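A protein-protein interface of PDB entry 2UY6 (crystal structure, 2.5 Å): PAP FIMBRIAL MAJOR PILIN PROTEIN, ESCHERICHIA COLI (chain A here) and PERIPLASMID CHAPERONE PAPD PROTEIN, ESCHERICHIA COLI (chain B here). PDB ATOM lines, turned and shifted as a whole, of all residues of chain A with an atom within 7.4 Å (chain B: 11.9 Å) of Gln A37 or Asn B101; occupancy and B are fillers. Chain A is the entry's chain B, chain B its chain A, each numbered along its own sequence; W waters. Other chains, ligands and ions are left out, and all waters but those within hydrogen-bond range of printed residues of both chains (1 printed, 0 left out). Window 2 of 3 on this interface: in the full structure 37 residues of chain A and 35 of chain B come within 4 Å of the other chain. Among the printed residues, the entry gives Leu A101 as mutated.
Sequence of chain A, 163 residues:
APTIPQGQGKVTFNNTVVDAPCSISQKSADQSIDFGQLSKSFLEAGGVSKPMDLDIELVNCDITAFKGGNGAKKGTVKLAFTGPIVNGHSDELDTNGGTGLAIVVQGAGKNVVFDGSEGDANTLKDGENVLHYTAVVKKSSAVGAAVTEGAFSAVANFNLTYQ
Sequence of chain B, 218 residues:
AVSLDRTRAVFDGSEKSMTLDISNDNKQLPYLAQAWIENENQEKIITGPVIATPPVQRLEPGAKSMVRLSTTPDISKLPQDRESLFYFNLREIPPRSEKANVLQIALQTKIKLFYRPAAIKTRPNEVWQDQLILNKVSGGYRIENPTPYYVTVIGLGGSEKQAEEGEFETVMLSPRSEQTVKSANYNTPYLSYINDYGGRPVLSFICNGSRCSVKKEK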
ATOM      1  N   ILE A  33      10.157  23.013   2.100  1.00  0.00           N
ATOM      2  CA  ILE A  33       9.247  22.389   1.156  1.00  0.00           C
ATOM      3  C   ILE A  33       9.300  20.912   1.514  1.00  0.00           C
ATOM      4  O   ILE A  33      10.373  20.351   1.748  1.00  0.00           O
ATOM      5  CB  ILE A  33       9.650  22.604  -0.317  1.00  0.00           C
ATOM      6  CG1 ILE A  33      11.100  22.191  -0.540  1.00  0.00           C
ATOM      7  CG2 ILE A  33       9.388  24.045  -0.711  1.00  0.00           C
ATOM      8  CD1 ILE A  33      11.505  22.238  -2.001  1.00  0.00           C
ATOM      9  N   ASP A  34       8.126  20.300   1.586  1.00  0.00           N
ATOM     10  CA  ASP A  34       7.983  18.902   1.953  1.00  0.00           C
ATOM     11  C   ASP A  34       7.852  18.045   0.702  1.00  0.00           C
ATOM     12  O   ASP A  34       7.048  18.340  -0.176  1.00  0.00           O
ATOM     13  CB  ASP A  34       6.746  18.791   2.850  1.00  0.00           C
ATOM     14  CG  ASP A  34       6.394  17.375   3.205  1.00  0.00           C
ATOM     15  OD1 ASP A  34       7.298  16.582   3.538  1.00  0.00           O
ATOM     16  OD2 ASP A  34       5.188  17.061   3.167  1.00  0.00           O
ATOM     17  N   PHE A  35       8.658  16.994   0.598  1.00  0.00           N
ATOM     18  CA  PHE A  35       8.580  16.120  -0.568  1.00  0.00           C
ATOM     19  C   PHE A  35       7.578  14.997  -0.356  1.00  0.00           C
ATOM     20  O   PHE A  35       7.376  14.169  -1.238  1.00  0.00           O
ATOM     21  CB  PHE A  35       9.942  15.515  -0.888  1.00  0.00           C
ATOM     22  CG  PHE A  35      10.979  16.528  -1.253  1.00  0.00           C
ATOM     23  CD1 PHE A  35      11.744  17.146  -0.270  1.00  0.00           C
ATOM     24  CD2 PHE A  35      11.182  16.881  -2.582  1.00  0.00           C
ATOM     25  CE1 PHE A  35      12.703  18.105  -0.609  1.00  0.00           C
ATOM     26  CE2 PHE A  35      12.138  17.838  -2.932  1.00  0.00           C
ATOM     27  CZ  PHE A  35      12.899  18.451  -1.944  1.00  0.00           C
ATOM     28  N   GLY A  36       6.947  14.977   0.815  1.00  0.00           N
ATOM     29  CA  GLY A  36       5.977  13.942   1.119  1.00  0.00           C
ATOM     30  C   GLY A  36       6.668  12.599   1.223  1.00  0.00           C
ATOM     31  O   GLY A  36       7.885  12.536   1.389  1.00  0.00           O
ATOM     32  N   GLN A  37       5.903  11.519   1.126  1.00  0.00           N
ATOM     33  CA  GLN A  37       6.498  10.191   1.203  1.00  0.00           C
ATOM     34  C   GLN A  37       6.969   9.722  -0.168  1.00  0.00           C
ATOM     35  O   GLN A  37       6.388  10.076  -1.190  1.00  0.00           O
ATOM     36  CB  GLN A  37       5.502   9.194   1.801  1.00  0.00           C
ATOM     37  CG  GLN A  37       5.130   9.516   3.245  1.00  0.00           C
ATOM     38  CD  GLN A  37       6.334   9.951   4.084  1.00  0.00           C
ATOM     39  OE1 GLN A  37       7.291   9.187   4.278  1.00  0.00           O
ATOM     40  NE2 GLN A  37       6.290  11.192   4.577  1.00  0.00           N
ATOM     41  N   LEU A  38       8.039   8.937  -0.180  1.00  0.00           N
ATOM     42  CA  LEU A  38       8.594   8.424  -1.424  1.00  0.00           C
ATOM     43  C   LEU A  38       8.942   6.940  -1.304  1.00  0.00           C
ATOM     44  O   LEU A  38       9.338   6.472  -0.237  1.00  0.00           O
ATOM     45  CB  LEU A  38       9.849   9.207  -1.796  1.00  0.00           C
ATOM     46  CG  LEU A  38       9.685  10.692  -2.093  1.00  0.00           C
ATOM     47  CD1 LEU A  38      11.068  11.310  -2.219  1.00  0.00           C
ATOM     48  CD2 LEU A  38       8.876  10.893  -3.372  1.00  0.00           C
ATOM     49  N   SER A  39       8.798   6.208  -2.407  1.00  0.00           N
ATOM     50  CA  SER A  39       9.100   4.785  -2.429  1.00  0.00           C
ATOM     51  C   SER A  39      10.593   4.530  -2.508  1.00  0.00           C
ATOM     52  O   SER A  39      11.259   4.971  -3.448  1.00  0.00           O
ATOM     53  CB  SER A  39       8.425   4.109  -3.623  1.00  0.00           C
ATOM     54  OG  SER A  39       9.043   2.860  -3.898  1.00  0.00           O
ATOM     55  N   LYS A  40      11.112   3.804  -1.523  1.00  0.00           N
ATOM     56  CA  LYS A  40      12.527   3.477  -1.490  1.00  0.00           C
ATOM     57  C   LYS A  40      12.884   2.718  -2.765  1.00  0.00           C
ATOM     58  O   LYS A  40      13.894   3.003  -3.415  1.00  0.00           O
ATOM     59  CB  LYS A  40      12.840   2.624  -0.255  1.00  0.00           C
ATOM     60  N   LEU A  43      12.816   5.115  -5.996  1.00  0.00           N
ATOM     61  CA  LEU A  43      14.021   5.928  -6.064  1.00  0.00           C
ATOM     62  C   LEU A  43      15.229   5.040  -6.328  1.00  0.00           C
ATOM     63  O   LEU A  43      16.133   5.416  -7.074  1.00  0.00           O
ATOM     64  CB  LEU A  43      14.247   6.701  -4.759  1.00  0.00           C
ATOM     65  CG  LEU A  43      13.551   8.046  -4.515  1.00  0.00           C
ATOM     66  CD1 LEU A  43      13.586   8.888  -5.795  1.00  0.00           C
ATOM     67  CD2 LEU A  43      12.128   7.824  -4.071  1.00  0.00           C
ATOM     68  N   SER A  49      11.606  11.970  -7.631  1.00  0.00           N
ATOM     69  CA  SER A  49      10.405  12.534  -7.027  1.00  0.00           C
ATOM     70  C   SER A  49       9.801  13.581  -7.963  1.00  0.00           C
ATOM     71  O   SER A  49      10.456  14.049  -8.901  1.00  0.00           O
ATOM     72  CB  SER A  49      10.743  13.202  -5.695  1.00  0.00           C
ATOM     73  OG  SER A  49      11.447  14.417  -5.909  1.00  0.00           O
ATOM     74  N   ASN A  96      20.417  14.604   4.965  1.00  0.00           N
ATOM     75  CA  ASN A  96      20.586  14.036   6.297  1.00  0.00           C
ATOM     76  C   ASN A  96      19.617  12.884   6.509  1.00  0.00           C
ATOM     77  O   ASN A  96      18.474  12.929   6.043  1.00  0.00           O
ATOM     78  CB  ASN A  96      20.324  15.085   7.380  1.00  0.00           C
ATOM     79  CG  ASN A  96      21.295  16.244   7.320  1.00  0.00           C
ATOM     80  OD1 ASN A  96      22.518  16.051   7.340  1.00  0.00           O
ATOM     81  ND2 ASN A  96      20.758  17.462   7.249  1.00  0.00           N
ATOM     82  N   THR A  99      19.781   8.110   4.177  1.00  0.00           N
ATOM     83  CA  THR A  99      18.874   7.410   3.280  1.00  0.00           C
ATOM     84  C   THR A  99      19.538   7.135   1.940  1.00  0.00           C
ATOM     85  O   THR A  99      19.077   6.290   1.179  1.00  0.00           O
ATOM     86  CB  THR A  99      17.600   8.231   3.014  1.00  0.00           C
ATOM     87  OG1 THR A  99      17.960   9.506   2.462  1.00  0.00           O
ATOM     88  CG2 THR A  99      16.805   8.432   4.300  1.00  0.00           C
ATOM     89  N   LEU A 101      19.766   9.407  -0.329  1.00  0.00           N
ATOM     90  CA  LEU A 101      19.169  10.319  -1.290  1.00  0.00           C
ATOM     91  C   LEU A 101      19.920  11.647  -1.395  1.00  0.00           C
ATOM     92  O   LEU A 101      20.696  12.024  -0.511  1.00  0.00           O
ATOM     93  CB  LEU A 101      17.714  10.581  -0.912  1.00  0.00           C
ATOM     94  CG  LEU A 101      16.855   9.331  -0.708  1.00  0.00           C
ATOM     95  CD1 LEU A 101      15.450   9.743  -0.273  1.00  0.00           C
ATOM     96  CD2 LEU A 101      16.817   8.517  -1.995  1.00  0.00           C
ATOM     97  N   ILE A 103      19.398  15.873  -3.224  1.00  0.00           N
ATOM     98  CA  ILE A 103      18.446  16.830  -3.775  1.00  0.00           C
ATOM     99  C   ILE A 103      19.051  17.641  -4.909  1.00  0.00           C
ATOM    100  O   ILE A 103      20.176  18.126  -4.812  1.00  0.00           O
ATOM    101  CB  ILE A 103      17.926  17.804  -2.701  1.00  0.00           C
ATOM    102  CG1 ILE A 103      17.167  17.031  -1.621  1.00  0.00           C
ATOM    103  CG2 ILE A 103      17.003  18.852  -3.345  1.00  0.00           C
ATOM    104  CD1 ILE A 103      16.617  17.906  -0.514  1.00  0.00           C
ATOM    105  N   VAL A 137      14.040  14.904  -5.498  1.00  0.00           N
ATOM    106  CA  VAL A 137      14.823  14.016  -4.650  1.00  0.00           C
ATOM    107  C   VAL A 137      15.157  12.764  -5.468  1.00  0.00           C
ATOM    108  O   VAL A 137      14.312  12.264  -6.214  1.00  0.00           O
ATOM    109  CB  VAL A 137      14.024  13.597  -3.397  1.00  0.00           C
ATOM    110  CG1 VAL A 137      14.822  12.584  -2.577  1.00  0.00           C
ATOM    111  CG2 VAL A 137      13.701  14.824  -2.565  1.00  0.00           C
ATOM    112  N   GLY A 150      13.566   5.567   5.689  1.00  0.00           N
ATOM    113  CA  GLY A 150      13.876   6.596   6.665  1.00  0.00           C
ATOM    114  C   GLY A 150      13.708   8.019   6.155  1.00  0.00           C
ATOM    115  O   GLY A 150      13.903   8.298   4.965  1.00  0.00           O
ATOM    116  N   ALA A 151      13.345   8.925   7.060  1.00  0.00           N
ATOM    117  CA  ALA A 151      13.154  10.331   6.719  1.00  0.00           C
ATOM    118  C   ALA A 151      14.487  11.048   6.492  1.00  0.00           C
ATOM    119  O   ALA A 151      15.477  10.784   7.176  1.00  0.00           O
ATOM    120  CB  ALA A 151      12.363  11.037   7.822  1.00  0.00           C
ATOM    121  N   PHE A 152      14.499  11.953   5.517  1.00  0.00           N
ATOM    122  CA  PHE A 152      15.692  12.726   5.187  1.00  0.00           C
ATOM    123  C   PHE A 152      15.364  14.209   5.341  1.00  0.00           C
ATOM    124  O   PHE A 152      14.197  14.584   5.511  1.00  0.00           O
ATOM    125  CB  PHE A 152      16.129  12.439   3.744  1.00  0.00           C
ATOM    126  CG  PHE A 152      15.139  12.900   2.709  1.00  0.00           C
ATOM    127  CD1 PHE A 152      15.118  14.223   2.284  1.00  0.00           C
ATOM    128  CD2 PHE A 152      14.206  12.018   2.184  1.00  0.00           C
ATOM    129  CE1 PHE A 152      14.178  14.659   1.346  1.00  0.00           C
ATOM    130  CE2 PHE A 152      13.265  12.444   1.250  1.00  0.00           C
ATOM    131  CZ  PHE A 152      13.250  13.766   0.830  1.00  0.00           C
ATOM    132  N   SER A 153      16.395  15.045   5.283  1.00  0.00           N
ATOM    133  CA  SER A 153      16.218  16.487   5.393  1.00  0.00           C
ATOM    134  C   SER A 153      17.473  17.153   4.872  1.00  0.00           C
ATOM    135  O   SER A 153      18.488  16.491   4.652  1.00  0.00           O
ATOM    136  CB  SER A 153      15.989  16.901   6.852  1.00  0.00           C
ATOM    137  OG  SER A 153      17.134  16.635   7.643  1.00  0.00           O
ATOM    138  N   ALA A 154      17.399  18.461   4.667  1.00  0.00           N
ATOM    139  CA  ALA A 154      18.547  19.220   4.191  1.00  0.00           C
ATOM    140  C   ALA A 154      18.307  20.714   4.325  1.00  0.00           C
ATOM    141  O   ALA A 154      17.161  21.172   4.418  1.00  0.00           O
ATOM    142  CB  ALA A 154      18.851  18.870   2.734  1.00  0.00           C
ATOM    143  N   ARG B  96      14.052  24.356  13.232  1.00  0.00           N
ATOM    144  CA  ARG B  96      14.036  22.983  12.719  1.00  0.00           C
ATOM    145  C   ARG B  96      12.621  22.652  12.236  1.00  0.00           C
ATOM    146  O   ARG B  96      11.641  22.970  12.912  1.00  0.00           O
ATOM    147  CB  ARG B  96      14.471  22.006  13.811  1.00  0.00           C
ATOM    148  N   SER B  97      12.512  22.026  11.067  1.00  0.00           N
ATOM    149  CA  SER B  97      11.200  21.686  10.521  1.00  0.00           C
ATOM    150  C   SER B  97      10.485  20.547  11.241  1.00  0.00           C
ATOM    151  O   SER B  97      11.108  19.628  11.796  1.00  0.00           O
ATOM    152  CB  SER B  97      11.303  21.335   9.032  1.00  0.00           C
ATOM    153  OG  SER B  97      10.013  21.107   8.476  1.00  0.00           O
ATOM    154  N   GLU B  98       9.159  20.626  11.221  1.00  0.00           N
ATOM    155  CA  GLU B  98       8.308  19.616  11.833  1.00  0.00           C
ATOM    156  C   GLU B  98       8.301  18.372  10.937  1.00  0.00           C
ATOM    157  O   GLU B  98       8.733  17.284  11.341  1.00  0.00           O
ATOM    158  CB  GLU B  98       6.884  20.164  11.960  1.00  0.00           C
ATOM    159  CG  GLU B  98       6.775  21.394  12.843  1.00  0.00           C
ATOM    160  CD  GLU B  98       6.981  21.065  14.310  1.00  0.00           C
ATOM    161  OE1 GLU B  98       6.002  20.652  14.975  1.00  0.00           O
ATOM    162  OE2 GLU B  98       8.126  21.203  14.790  1.00  0.00           O
ATOM    163  N   LYS B  99       7.812  18.563   9.714  1.00  0.00           N
ATOM    164  CA  LYS B  99       7.710  17.502   8.718  1.00  0.00           C
ATOM    165  C   LYS B  99       9.026  16.751   8.511  1.00  0.00           C
ATOM    166  O   LYS B  99      10.097  17.216   8.896  1.00  0.00           O
ATOM    167  CB  LYS B  99       7.281  18.097   7.380  1.00  0.00           C
ATOM    168  CG  LYS B  99       6.152  19.114   7.446  1.00  0.00           C
ATOM    169  CD  LYS B  99       6.046  19.881   6.129  1.00  0.00           C
ATOM    170  CE  LYS B  99       4.825  20.788   6.107  1.00  0.00           C
ATOM    171  NZ  LYS B  99       3.539  20.028   6.175  1.00  0.00           N
ATOM    172  N   ALA B 100       8.925  15.585   7.886  1.00  0.00           N
ATOM    173  CA  ALA B 100      10.073  14.757   7.577  1.00  0.00           C
ATOM    174  C   ALA B 100      10.211  14.885   6.067  1.00  0.00           C
ATOM    175  O   ALA B 100       9.236  15.195   5.386  1.00  0.00           O
ATOM    176  CB  ALA B 100       9.786  13.327   7.964  1.00  0.00           C
ATOM    177  N   ASN B 101      11.408  14.645   5.544  1.00  0.00           N
ATOM    178  CA  ASN B 101      11.659  14.767   4.104  1.00  0.00           C
ATOM    179  C   ASN B 101      11.418  16.215   3.671  1.00  0.00           C
ATOM    180  O   ASN B 101      10.528  16.518   2.865  1.00  0.00           O
ATOM    181  CB  ASN B 101      10.747  13.842   3.301  1.00  0.00           C
ATOM    182  CG  ASN B 101      10.844  12.409   3.752  1.00  0.00           C
ATOM    183  OD1 ASN B 101      11.927  11.930   4.109  1.00  0.00           O
ATOM    184  ND2 ASN B 101       9.723  11.701   3.708  1.00  0.00           N
ATOM    185  N   VAL B 102      12.227  17.114   4.210  1.00  0.00           N
ATOM    186  CA  VAL B 102      12.078  18.515   3.900  1.00  0.00           C
ATOM    187  C   VAL B 102      13.413  19.169   3.557  1.00  0.00           C
ATOM    188  O   VAL B 102      14.489  18.690   3.938  1.00  0.00           O
ATOM    189  CB  VAL B 102      11.392  19.243   5.086  1.00  0.00           C
ATOM    190  CG1 VAL B 102      12.392  19.512   6.179  1.00  0.00           C
ATOM    191  CG2 VAL B 102      10.754  20.521   4.617  1.00  0.00           C
ATOM    192  N   LEU B 103      13.316  20.254   2.799  1.00  0.00           N
ATOM    193  CA  LEU B 103      14.466  21.040   2.368  1.00  0.00           C
ATOM    194  C   LEU B 103      14.156  22.437   2.885  1.00  0.00           C
ATOM    195  O   LEU B 103      13.041  22.922   2.701  1.00  0.00           O
ATOM    196  CB  LEU B 103      14.543  21.062   0.832  1.00  0.00           C
ATOM    197  CG  LEU B 103      15.789  21.567   0.084  1.00  0.00           C
ATOM    198  CD1 LEU B 103      15.407  22.733  -0.805  1.00  0.00           C
ATOM    199  CD2 LEU B 103      16.893  21.965   1.053  1.00  0.00           C
ATOM    200  N   GLN B 104      15.118  23.064   3.557  1.00  0.00           N
ATOM    201  CA  GLN B 104      14.912  24.414   4.061  1.00  0.00           C
ATOM    202  C   GLN B 104      15.922  25.397   3.465  1.00  0.00           C
ATOM    203  O   GLN B 104      17.081  25.049   3.211  1.00  0.00           O
ATOM    204  CB  GLN B 104      14.997  24.444   5.590  1.00  0.00           C
ATOM    205  CG  GLN B 104      14.001  23.534   6.270  1.00  0.00           C
ATOM    206  CD  GLN B 104      14.003  23.674   7.775  1.00  0.00           C
ATOM    207  OE1 GLN B 104      13.438  24.621   8.318  1.00  0.00           O
ATOM    208  NE2 GLN B 104      14.646  22.730   8.462  1.00  0.00           N
ATOM    209  N   ILE B 105      15.466  26.626   3.234  1.00  0.00           N
ATOM    210  CA  ILE B 105      16.303  27.687   2.685  1.00  0.00           C
ATOM    211  C   ILE B 105      16.725  28.667   3.789  1.00  0.00           C
ATOM    212  O   ILE B 105      15.900  29.107   4.594  1.00  0.00           O
ATOM    213  CB  ILE B 105      15.543  28.468   1.590  1.00  0.00           C
ATOM    214  CG1 ILE B 105      15.239  27.546   0.410  1.00  0.00           C
ATOM    215  CG2 ILE B 105      16.358  29.673   1.133  1.00  0.00           C
ATOM    216  CD1 ILE B 105      16.456  26.849  -0.159  1.00  0.00           C
HETATM  217  O   HOH W   1      15.880  20.878   7.038  1.00  0.00           O
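O of Asn B101 lies within hydrogen-bond range of N of Phe A35 (3.0 Å). The side-chain amide nitrogen (ND2) of Asn B101 is in hydrogen-bond range of the backbone carbonyl oxygen (O) of Gly A36, at 3.1 Å. N of Asn B101 is in hydrogen-bond range of O of Phe A152, at 2.8 Å. N of Val B102 sits at hydrogen-bond distance from O of Phe A152. O of Val B102 sits at hydrogen-bond distance from N of Ala A154, 3.0 Å away. The backbone carbonyl oxygen (O) of Leu B103 sits at hydrogen-bond distance from the backbone NH (N) of Ile A33, 2.9 Å away. The backbone NH of Gln B104 lies within hydrogen-bond range of the backbone carbonyl oxygen of Ala A154 (2.9 Å). The side-chain carboxylate of Asp A34 sits close to the backbone carbonyl oxygen of Ala B100, at 3.0 Å. The side-chain carboxylate of Asp A34 lies close to the backbone carbonyl oxygen of Asn B101 (3.3 Å).
The side-chain amide nitrogen of Gln B104 lies close to the backbone NH of Ser B97 (3.4 Å). The side-chain carboxylate of Asp A34 sits at hydrogen-bond distance from the backbone NH of Gly A36 (3.2 Å). N of Asn A96 is in hydrogen-bond range of O of Ser A153, 2.7 Å away.
O of Ile A33 touches O of Asn B101, 3.995 Å away. Val B102 touches Ile A33. Lys B99 touches Asp A34 (CD to CB, 3.5 Å). Phe A35 touches Leu B103. Asn B101 touches Gln A37. Leu B103 touches Ile A103. Ala B100 touches Ala A151 (CB to CB, 3.5 Å). OD1 of Asn B101 touches CA of Ala A151, 3.3 Å away. Ser A153 touches Val B102. Leu B103 touches Ala A154 (CA to O, 3.4 Å).
Gln A37 touches just one residue of chain B: Asn B101. Phe A35 touches just these residues of chain B: Asn B101 (3.0 Å) and Leu B103 (3.8 Å). Of the printed residues of chain B, Gly A36 touches Asn B101 (3.1 Å). Leu A38 touches none of the printed residues of chain B. Ala A151 touches two residues of chain B. Of the printed residues of chain B, Phe A152 touches Asn B101 (2.8 Å) and Val B102 (3.5 Å). Of the printed residues of chain B, Ile A33 touches Asn B101, Val B102 and Leu B103. Of the printed residues of chain B, Asp A34 touches Lys B99 (3.5 Å), Ala B100 (3.0 Å) and Asn B101 (3.3 Å). Of the printed residues of chain B, Ile A103 touches Leu B103 (3.8 Å). Printed residues of chain B within 4 Å of Ala A154: Val B102, Leu B103 and Gln B104. Of the printed residues of chain A, Gln B104 touches Ala A154 (2.9 Å). Leu A43 touches none of the printed residues of chain B. The nearest residue of chain B that does not touch Gln A37 is Ala B100 (5.0 Å). The nearest printed residue of chain A that does not touch Asn B101 is Gly A150 (4.2 Å).
Of the 20 printed residues of chain A, 10 touch a printed residue of chain B. Hydrophobic or aromatic side chains of chain A that line the printed part of chain B: Ile A33, Phe A35, Ile A103, Ala A151 and Phe A152. Of the 10 printed residues of chain B, 6 touch a printed residue of chain A. Printed residues of chain B that touch a printed residue of chain A: Lys B99, Ala B100, Asn B101, Val B102, Leu B103 and Gln B104. Hydrophobic or aromatic side chains of chain B within 4 Å of the printed part of chain A: Ala B100, Val B102 and Leu B103. Among the printed residues, no Asp or Glu carboxylate lies within 4 Å of a Lys or Arg side-chain nitrogen of the other chain.
Water W1 lies within hydrogen-bond range of NE2 of Gln B104 (2.6 Å) and O of Ala A154 (2.9 Å).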
